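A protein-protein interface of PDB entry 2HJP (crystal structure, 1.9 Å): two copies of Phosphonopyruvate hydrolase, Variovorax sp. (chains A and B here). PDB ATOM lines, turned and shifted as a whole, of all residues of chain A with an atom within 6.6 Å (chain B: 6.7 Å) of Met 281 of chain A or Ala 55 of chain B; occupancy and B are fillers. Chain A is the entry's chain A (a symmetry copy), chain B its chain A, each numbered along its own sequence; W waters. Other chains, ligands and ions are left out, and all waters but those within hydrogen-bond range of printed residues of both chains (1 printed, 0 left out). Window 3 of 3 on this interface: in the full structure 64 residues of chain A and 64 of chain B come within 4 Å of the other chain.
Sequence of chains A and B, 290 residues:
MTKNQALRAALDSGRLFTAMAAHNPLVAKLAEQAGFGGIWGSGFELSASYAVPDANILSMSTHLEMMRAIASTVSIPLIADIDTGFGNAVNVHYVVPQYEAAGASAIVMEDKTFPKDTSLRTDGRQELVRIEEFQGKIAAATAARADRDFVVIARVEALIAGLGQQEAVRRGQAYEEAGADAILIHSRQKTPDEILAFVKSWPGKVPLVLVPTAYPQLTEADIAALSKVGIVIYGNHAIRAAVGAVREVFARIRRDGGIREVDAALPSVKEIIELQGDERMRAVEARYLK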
ATOM      1  N   ILE A 273     -13.449  32.406 -10.054  1.00  0.00           N
ATOM      2  CA  ILE A 273     -13.588  31.355 -11.049  1.00  0.00           C
ATOM      3  C   ILE A 273     -12.548  30.214 -10.829  1.00  0.00           C
ATOM      4  O   ILE A 273     -12.831  29.027 -11.080  1.00  0.00           O
ATOM      5  CB  ILE A 273     -13.479  31.973 -12.502  1.00  0.00           C
ATOM      6  CG1 ILE A 273     -14.778  32.769 -12.773  1.00  0.00           C
ATOM      7  CG2 ILE A 273     -13.409  30.874 -13.587  1.00  0.00           C
ATOM      8  CD1 ILE A 273     -14.695  33.762 -13.932  1.00  0.00           C
ATOM      9  N   GLN A 276     -13.607  28.024  -8.070  1.00  0.00           N
ATOM     10  CA  GLN A 276     -14.700  27.182  -8.522  1.00  0.00           C
ATOM     11  C   GLN A 276     -14.260  25.914  -9.273  1.00  0.00           C
ATOM     12  O   GLN A 276     -15.084  25.104  -9.641  1.00  0.00           O
ATOM     13  CB  GLN A 276     -15.613  28.004  -9.446  1.00  0.00           C
ATOM     14  CG  GLN A 276     -16.610  28.934  -8.720  1.00  0.00           C
ATOM     15  CD  GLN A 276     -17.314  29.835  -9.756  1.00  0.00           C
ATOM     16  OE1 GLN A 276     -16.641  30.548 -10.546  1.00  0.00           O
ATOM     17  NE2 GLN A 276     -18.650  29.788  -9.787  1.00  0.00           N
ATOM     18  N   GLY A 277     -12.967  25.756  -9.516  1.00  0.00           N
ATOM     19  CA  GLY A 277     -12.490  24.568 -10.208  1.00  0.00           C
ATOM     20  C   GLY A 277     -12.525  24.742 -11.726  1.00  0.00           C
ATOM     21  O   GLY A 277     -12.618  23.738 -12.480  1.00  0.00           O
ATOM     22  N   ASP A 278     -12.429  25.995 -12.188  1.00  0.00           N
ATOM     23  CA  ASP A 278     -12.452  26.237 -13.621  1.00  0.00           C
ATOM     24  C   ASP A 278     -11.423  25.401 -14.389  1.00  0.00           C
ATOM     25  O   ASP A 278     -11.705  24.894 -15.457  1.00  0.00           O
ATOM     26  CB  ASP A 278     -12.217  27.702 -13.904  1.00  0.00           C
ATOM     27  CG  ASP A 278     -12.547  28.070 -15.335  1.00  0.00           C
ATOM     28  OD1 ASP A 278     -13.762  27.944 -15.704  1.00  0.00           O
ATOM     29  OD2 ASP A 278     -11.569  28.479 -16.042  1.00  0.00           O
ATOM     30  N   GLU A 279     -10.224  25.284 -13.839  1.00  0.00           N
ATOM     31  CA  GLU A 279      -9.146  24.530 -14.457  1.00  0.00           C
ATOM     32  C   GLU A 279      -9.559  23.086 -14.790  1.00  0.00           C
ATOM     33  O   GLU A 279      -9.429  22.599 -15.925  1.00  0.00           O
ATOM     34  CB  GLU A 279      -7.962  24.505 -13.489  1.00  0.00           C
ATOM     35  CG  GLU A 279      -6.955  25.604 -13.689  1.00  0.00           C
ATOM     36  CD  GLU A 279      -5.866  25.162 -14.641  1.00  0.00           C
ATOM     37  OE1 GLU A 279      -6.116  25.212 -15.881  1.00  0.00           O
ATOM     38  OE2 GLU A 279      -4.771  24.736 -14.161  1.00  0.00           O
ATOM     39  N   ARG A 280     -10.037  22.407 -13.761  1.00  0.00           N
ATOM     40  CA  ARG A 280     -10.500  21.055 -13.915  1.00  0.00           C
ATOM     41  C   ARG A 280     -11.592  21.012 -14.995  1.00  0.00           C
ATOM     42  O   ARG A 280     -11.549  20.203 -15.918  1.00  0.00           O
ATOM     43  CB  ARG A 280     -11.023  20.534 -12.573  1.00  0.00           C
ATOM     44  CG  ARG A 280     -11.571  19.116 -12.693  1.00  0.00           C
ATOM     45  CD  ARG A 280     -11.898  18.475 -11.361  1.00  0.00           C
ATOM     46  NE  ARG A 280     -13.337  18.236 -11.200  1.00  0.00           N
ATOM     47  CZ  ARG A 280     -13.866  17.073 -10.841  1.00  0.00           C
ATOM     48  NH1 ARG A 280     -13.082  16.020 -10.613  1.00  0.00           N
ATOM     49  NH2 ARG A 280     -15.181  16.972 -10.675  1.00  0.00           N
ATOM     50  N   MET A 281     -12.558  21.909 -14.897  1.00  0.00           N
ATOM     51  CA  MET A 281     -13.609  21.936 -15.870  1.00  0.00           C
ATOM     52  C   MET A 281     -13.066  22.137 -17.284  1.00  0.00           C
ATOM     53  O   MET A 281     -13.581  21.525 -18.225  1.00  0.00           O
ATOM     54  CB  MET A 281     -14.676  23.009 -15.540  1.00  0.00           C
ATOM     55  CG  MET A 281     -15.844  22.994 -16.544  1.00  0.00           C
ATOM     56  SD  MET A 281     -17.062  24.281 -16.394  1.00  0.00           S
ATOM     57  CE  MET A 281     -16.018  25.767 -16.549  1.00  0.00           C
ATOM     58  N   ARG A 282     -12.047  22.986 -17.480  1.00  0.00           N
ATOM     59  CA  ARG A 282     -11.508  23.135 -18.865  1.00  0.00           C
ATOM     60  C   ARG A 282     -10.842  21.849 -19.366  1.00  0.00           C
ATOM     61  O   ARG A 282     -10.861  21.532 -20.566  1.00  0.00           O
ATOM     62  CB  ARG A 282     -10.518  24.358 -18.968  1.00  0.00           C
ATOM     63  CG  ARG A 282     -11.311  25.694 -18.883  1.00  0.00           C
ATOM     64  CD  ARG A 282     -10.404  26.950 -18.924  1.00  0.00           C
ATOM     65  NE  ARG A 282      -9.179  26.621 -18.203  1.00  0.00           N
ATOM     66  CZ  ARG A 282      -8.448  27.470 -17.490  1.00  0.00           C
ATOM     67  NH1 ARG A 282      -8.797  28.760 -17.379  1.00  0.00           N
ATOM     68  NH2 ARG A 282      -7.374  27.012 -16.861  1.00  0.00           N
ATOM     69  N   ALA A 283     -10.234  21.103 -18.457  1.00  0.00           N
ATOM     70  CA  ALA A 283      -9.597  19.842 -18.862  1.00  0.00           C
ATOM     71  C   ALA A 283     -10.724  18.893 -19.293  1.00  0.00           C
ATOM     72  O   ALA A 283     -10.645  18.239 -20.368  1.00  0.00           O
ATOM     73  CB  ALA A 283      -8.795  19.272 -17.703  1.00  0.00           C
ATOM     74  N   VAL A 284     -11.813  18.863 -18.509  1.00  0.00           N
ATOM     75  CA  VAL A 284     -12.932  18.002 -18.858  1.00  0.00           C
ATOM     76  C   VAL A 284     -13.542  18.400 -20.223  1.00  0.00           C
ATOM     77  O   VAL A 284     -13.783  17.529 -21.104  1.00  0.00           O
ATOM     78  CB  VAL A 284     -13.980  17.980 -17.717  1.00  0.00           C
ATOM     79  CG1 VAL A 284     -15.330  17.312 -18.202  1.00  0.00           C
ATOM     80  CG2 VAL A 284     -13.461  17.119 -16.562  1.00  0.00           C
ATOM     81  N   GLU A 285     -13.778  19.689 -20.439  1.00  0.00           N
ATOM     82  CA  GLU A 285     -14.340  20.133 -21.710  1.00  0.00           C
ATOM     83  C   GLU A 285     -13.405  19.783 -22.826  1.00  0.00           C
ATOM     84  O   GLU A 285     -13.833  19.334 -23.908  1.00  0.00           O
ATOM     85  CB  GLU A 285     -14.521  21.647 -21.819  1.00  0.00           C
ATOM     86  CG  GLU A 285     -15.490  22.239 -20.905  1.00  0.00           C
ATOM     87  CD  GLU A 285     -15.861  23.678 -21.309  1.00  0.00           C
ATOM     88  OE1 GLU A 285     -15.896  24.013 -22.518  1.00  0.00           O
ATOM     89  OE2 GLU A 285     -16.146  24.455 -20.388  1.00  0.00           O
ATOM     90  N   ALA A 286     -12.118  20.040 -22.593  1.00  0.00           N
ATOM     91  CA  ALA A 286     -11.136  19.740 -23.644  1.00  0.00           C
ATOM     92  C   ALA A 286     -11.094  18.250 -23.946  1.00  0.00           C
ATOM     93  O   ALA A 286     -10.952  17.873 -25.101  1.00  0.00           O
ATOM     94  CB  ALA A 286      -9.765  20.206 -23.244  1.00  0.00           C
ATOM     95  N   SER B  47     -23.277  29.161  -7.345  1.00  0.00           N
ATOM     96  CA  SER B  47     -22.358  28.097  -7.763  1.00  0.00           C
ATOM     97  C   SER B  47     -20.962  28.366  -7.161  1.00  0.00           C
ATOM     98  O   SER B  47     -20.263  27.452  -6.773  1.00  0.00           O
ATOM     99  CB  SER B  47     -22.294  27.978  -9.326  1.00  0.00           C
ATOM    100  OG  SER B  47     -21.827  29.228  -9.794  1.00  0.00           O
ATOM    101  N   VAL B  52     -18.211  25.225  -7.541  1.00  0.00           N
ATOM    102  CA  VAL B  52     -18.418  24.570  -8.848  1.00  0.00           C
ATOM    103  C   VAL B  52     -18.569  25.696  -9.883  1.00  0.00           C
ATOM    104  O   VAL B  52     -18.964  26.829  -9.528  1.00  0.00           O
ATOM    105  CB  VAL B  52     -19.641  23.593  -8.885  1.00  0.00           C
ATOM    106  CG1 VAL B  52     -19.394  22.453  -7.922  1.00  0.00           C
ATOM    107  CG2 VAL B  52     -20.983  24.344  -8.676  1.00  0.00           C
ATOM    108  N   PRO B  53     -18.198  25.428 -11.166  1.00  0.00           N
ATOM    109  CA  PRO B  53     -18.312  26.477 -12.175  1.00  0.00           C
ATOM    110  C   PRO B  53     -19.742  26.889 -12.450  1.00  0.00           C
ATOM    111  O   PRO B  53     -20.663  26.107 -12.222  1.00  0.00           O
ATOM    112  CB  PRO B  53     -17.659  25.865 -13.442  1.00  0.00           C
ATOM    113  CG  PRO B  53     -16.712  24.797 -12.886  1.00  0.00           C
ATOM    114  CD  PRO B  53     -17.523  24.233 -11.707  1.00  0.00           C
ATOM    115  N   ASP B  54     -19.894  28.135 -12.913  1.00  0.00           N
ATOM    116  CA  ASP B  54     -21.195  28.700 -13.293  1.00  0.00           C
ATOM    117  C   ASP B  54     -21.423  28.229 -14.772  1.00  0.00           C
ATOM    118  O   ASP B  54     -21.335  29.035 -15.682  1.00  0.00           O
ATOM    119  CB  ASP B  54     -21.113  30.240 -13.192  1.00  0.00           C
ATOM    120  CG  ASP B  54     -22.440  30.938 -13.532  1.00  0.00           C
ATOM    121  OD1 ASP B  54     -22.406  32.137 -13.943  1.00  0.00           O
ATOM    122  OD2 ASP B  54     -23.499  30.284 -13.388  1.00  0.00           O
ATOM    123  N   ALA B  55     -21.669  26.935 -14.981  1.00  0.00           N
ATOM    124  CA  ALA B  55     -21.836  26.377 -16.314  1.00  0.00           C
ATOM    125  C   ALA B  55     -22.937  25.338 -16.229  1.00  0.00           C
ATOM    126  O   ALA B  55     -22.776  24.200 -16.687  1.00  0.00           O
ATOM    127  CB  ALA B  55     -20.516  25.707 -16.768  1.00  0.00           C
ATOM    128  N   ASN B  56     -24.042  25.717 -15.593  1.00  0.00           N
ATOM    129  CA  ASN B  56     -25.194  24.826 -15.424  1.00  0.00           C
ATOM    130  C   ASN B  56     -24.813  23.507 -14.740  1.00  0.00           C
ATOM    131  O   ASN B  56     -25.361  22.431 -15.022  1.00  0.00           O
ATOM    132  CB  ASN B  56     -25.873  24.533 -16.765  1.00  0.00           C
ATOM    133  CG  ASN B  56     -25.958  25.774 -17.689  1.00  0.00           C
ATOM    134  OD1 ASN B  56     -25.123  25.978 -18.610  1.00  0.00           O
ATOM    135  ND2 ASN B  56     -26.953  26.596 -17.454  1.00  0.00           N
ATOM    136  N   ILE B  57     -23.883  23.580 -13.815  1.00  0.00           N
ATOM    137  CA  ILE B  57     -23.516  22.361 -13.126  1.00  0.00           C
ATOM    138  C   ILE B  57     -24.314  22.240 -11.876  1.00  0.00           C
ATOM    139  O   ILE B  57     -24.753  21.181 -11.520  1.00  0.00           O
ATOM    140  CB  ILE B  57     -22.014  22.362 -12.808  1.00  0.00           C
ATOM    141  CG1 ILE B  57     -21.264  22.139 -14.120  1.00  0.00           C
ATOM    142  CG2 ILE B  57     -21.708  21.263 -11.740  1.00  0.00           C
ATOM    143  CD1 ILE B  57     -19.759  22.367 -14.039  1.00  0.00           C
ATOM    144  N   LEU B  58     -24.521  23.365 -11.202  1.00  0.00           N
ATOM    145  CA  LEU B  58     -25.267  23.365  -9.958  1.00  0.00           C
ATOM    146  C   LEU B  58     -26.697  22.924 -10.203  1.00  0.00           C
ATOM    147  O   LEU B  58     -27.314  23.347 -11.174  1.00  0.00           O
ATOM    148  CB  LEU B  58     -25.264  24.789  -9.400  1.00  0.00           C
ATOM    149  CG  LEU B  58     -25.822  24.942  -8.004  1.00  0.00           C
ATOM    150  CD1 LEU B  58     -24.790  24.456  -6.921  1.00  0.00           C
ATOM    151  CD2 LEU B  58     -26.175  26.399  -7.866  1.00  0.00           C
ATOM    152  N   ASP B  83     -30.765  31.197 -15.485  1.00  0.00           N
ATOM    153  CA  ASP B  83     -29.835  30.831 -16.556  1.00  0.00           C
ATOM    154  C   ASP B  83     -30.538  30.792 -17.906  1.00  0.00           C
ATOM    155  O   ASP B  83     -31.043  31.840 -18.327  1.00  0.00           O
ATOM    156  CB  ASP B  83     -29.181  29.475 -16.249  1.00  0.00           C
ATOM    157  CG  ASP B  83     -28.116  29.549 -15.087  1.00  0.00           C
ATOM    158  OD1 ASP B  83     -27.386  28.523 -14.932  1.00  0.00           O
ATOM    159  OD2 ASP B  83     -28.001  30.570 -14.313  1.00  0.00           O
ATOM    160  N   PHE B 114     -28.120  25.909 -24.869  1.00  0.00           N
ATOM    161  CA  PHE B 114     -27.805  25.104 -23.715  1.00  0.00           C
ATOM    162  C   PHE B 114     -28.156  23.688 -24.060  1.00  0.00           C
ATOM    163  O   PHE B 114     -29.218  23.440 -24.561  1.00  0.00           O
ATOM    164  CB  PHE B 114     -28.645  25.508 -22.517  1.00  0.00           C
ATOM    165  CG  PHE B 114     -28.691  24.455 -21.466  1.00  0.00           C
ATOM    166  CD1 PHE B 114     -27.577  24.240 -20.654  1.00  0.00           C
ATOM    167  CD2 PHE B 114     -29.773  23.553 -21.417  1.00  0.00           C
ATOM    168  CE1 PHE B 114     -27.506  23.138 -19.815  1.00  0.00           C
ATOM    169  CE2 PHE B 114     -29.739  22.443 -20.590  1.00  0.00           C
ATOM    170  CZ  PHE B 114     -28.605  22.214 -19.779  1.00  0.00           C
ATOM    171  N   LYS B 116     -23.824  23.937 -23.642  1.00  0.00           N
ATOM    172  CA  LYS B 116     -22.753  24.435 -24.489  1.00  0.00           C
ATOM    173  C   LYS B 116     -22.283  23.365 -25.494  1.00  0.00           C
ATOM    174  O   LYS B 116     -22.173  22.144 -25.196  1.00  0.00           O
ATOM    175  CB  LYS B 116     -21.574  24.909 -23.618  1.00  0.00           C
ATOM    176  CG  LYS B 116     -20.253  25.107 -24.395  1.00  0.00           C
ATOM    177  CD  LYS B 116     -19.414  26.315 -23.929  1.00  0.00           C
ATOM    178  CE  LYS B 116     -18.246  25.967 -23.013  1.00  0.00           C
ATOM    179  NZ  LYS B 116     -17.203  27.081 -22.910  1.00  0.00           N
HETATM  180  O   HOH W   1     -17.446  29.903 -12.830  1.00  0.00           O
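The side-chain amide nitrogen of Gln 276 of chain A is in hydrogen-bond range of the side-chain hydroxyl of Ser 47 of chain B. The side-chain amide nitrogen of Gln 276 of chain A sits at hydrogen-bond distance from the backbone carbonyl oxygen of Val 52 of chain B, 3.0 Å away. The side-chain carboxylate (OE1) of Glu 285 of chain A is in salt-bridge range of the side-chain amino group (NZ) of Lys 116 of chain B, 3.4 Å away. O of Gln 276 of chain A sits close to N of Pro 53 of chain B.
O of Ser 47 of chain B is in hydrogen-bond range of N of Val 52 of chain B (3.1 Å).
NE2 of Gln 276 of chain A touches N of Asp 54 of chain B (3.7 Å). Pro 53 of chain B touches Met 281 of chain A (CB to SD, 3.4 Å). SD of Met 281 of chain A touches CB of Ala 55 of chain B, 3.8 Å away.
Of the printed residues of chain B, Gln 276 of chain A touches Ser 47, Val 52, Pro 53 and Asp 54. Of chain B, only Pro 53 and Ala 55 come within 4 Å of Met 281 of chain A. Of the printed residues of chain A, Pro 53 of chain B touches Gln 276 (3.3 Å) and Met 281 (3.4 Å). Ala 55 of chain B touches one residue of chain A. Phe 114 of chain B touches none of the printed residues of chain A. Printed residues of chain A within 4 Å of Lys 116 of chain B: Glu 285 (3.1 Å). The nearest residue of chain A that does not touch Ala 55 of chain B is Glu 285 of chain A (5.8 Å).
Of the 12 printed residues of chain A, 3 touch a printed residue of chain B. Hydrophobic or aromatic side chains of chain A that line the printed part of chain B: Met 281. Of the 11 printed residues of chain B, 6 touch a printed residue of chain A. Along chain B the printed residues that touch a printed residue of chain A span positions 47 to 116. Among the printed residues, 7 pairs touch across the chains. Among the printed residues, Asp or Glu carboxylates within 4 Å of a Lys or Arg side-chain nitrogen of the other chain: Glu 285 of chain A with Lys 116 of chain B (3.4 Å).
No position is printed for both chains.
Water W1 bridges OE1 of Gln 276 of chain A (2.5 Å) and N of Asp 54 of chain B (3.0 Å).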
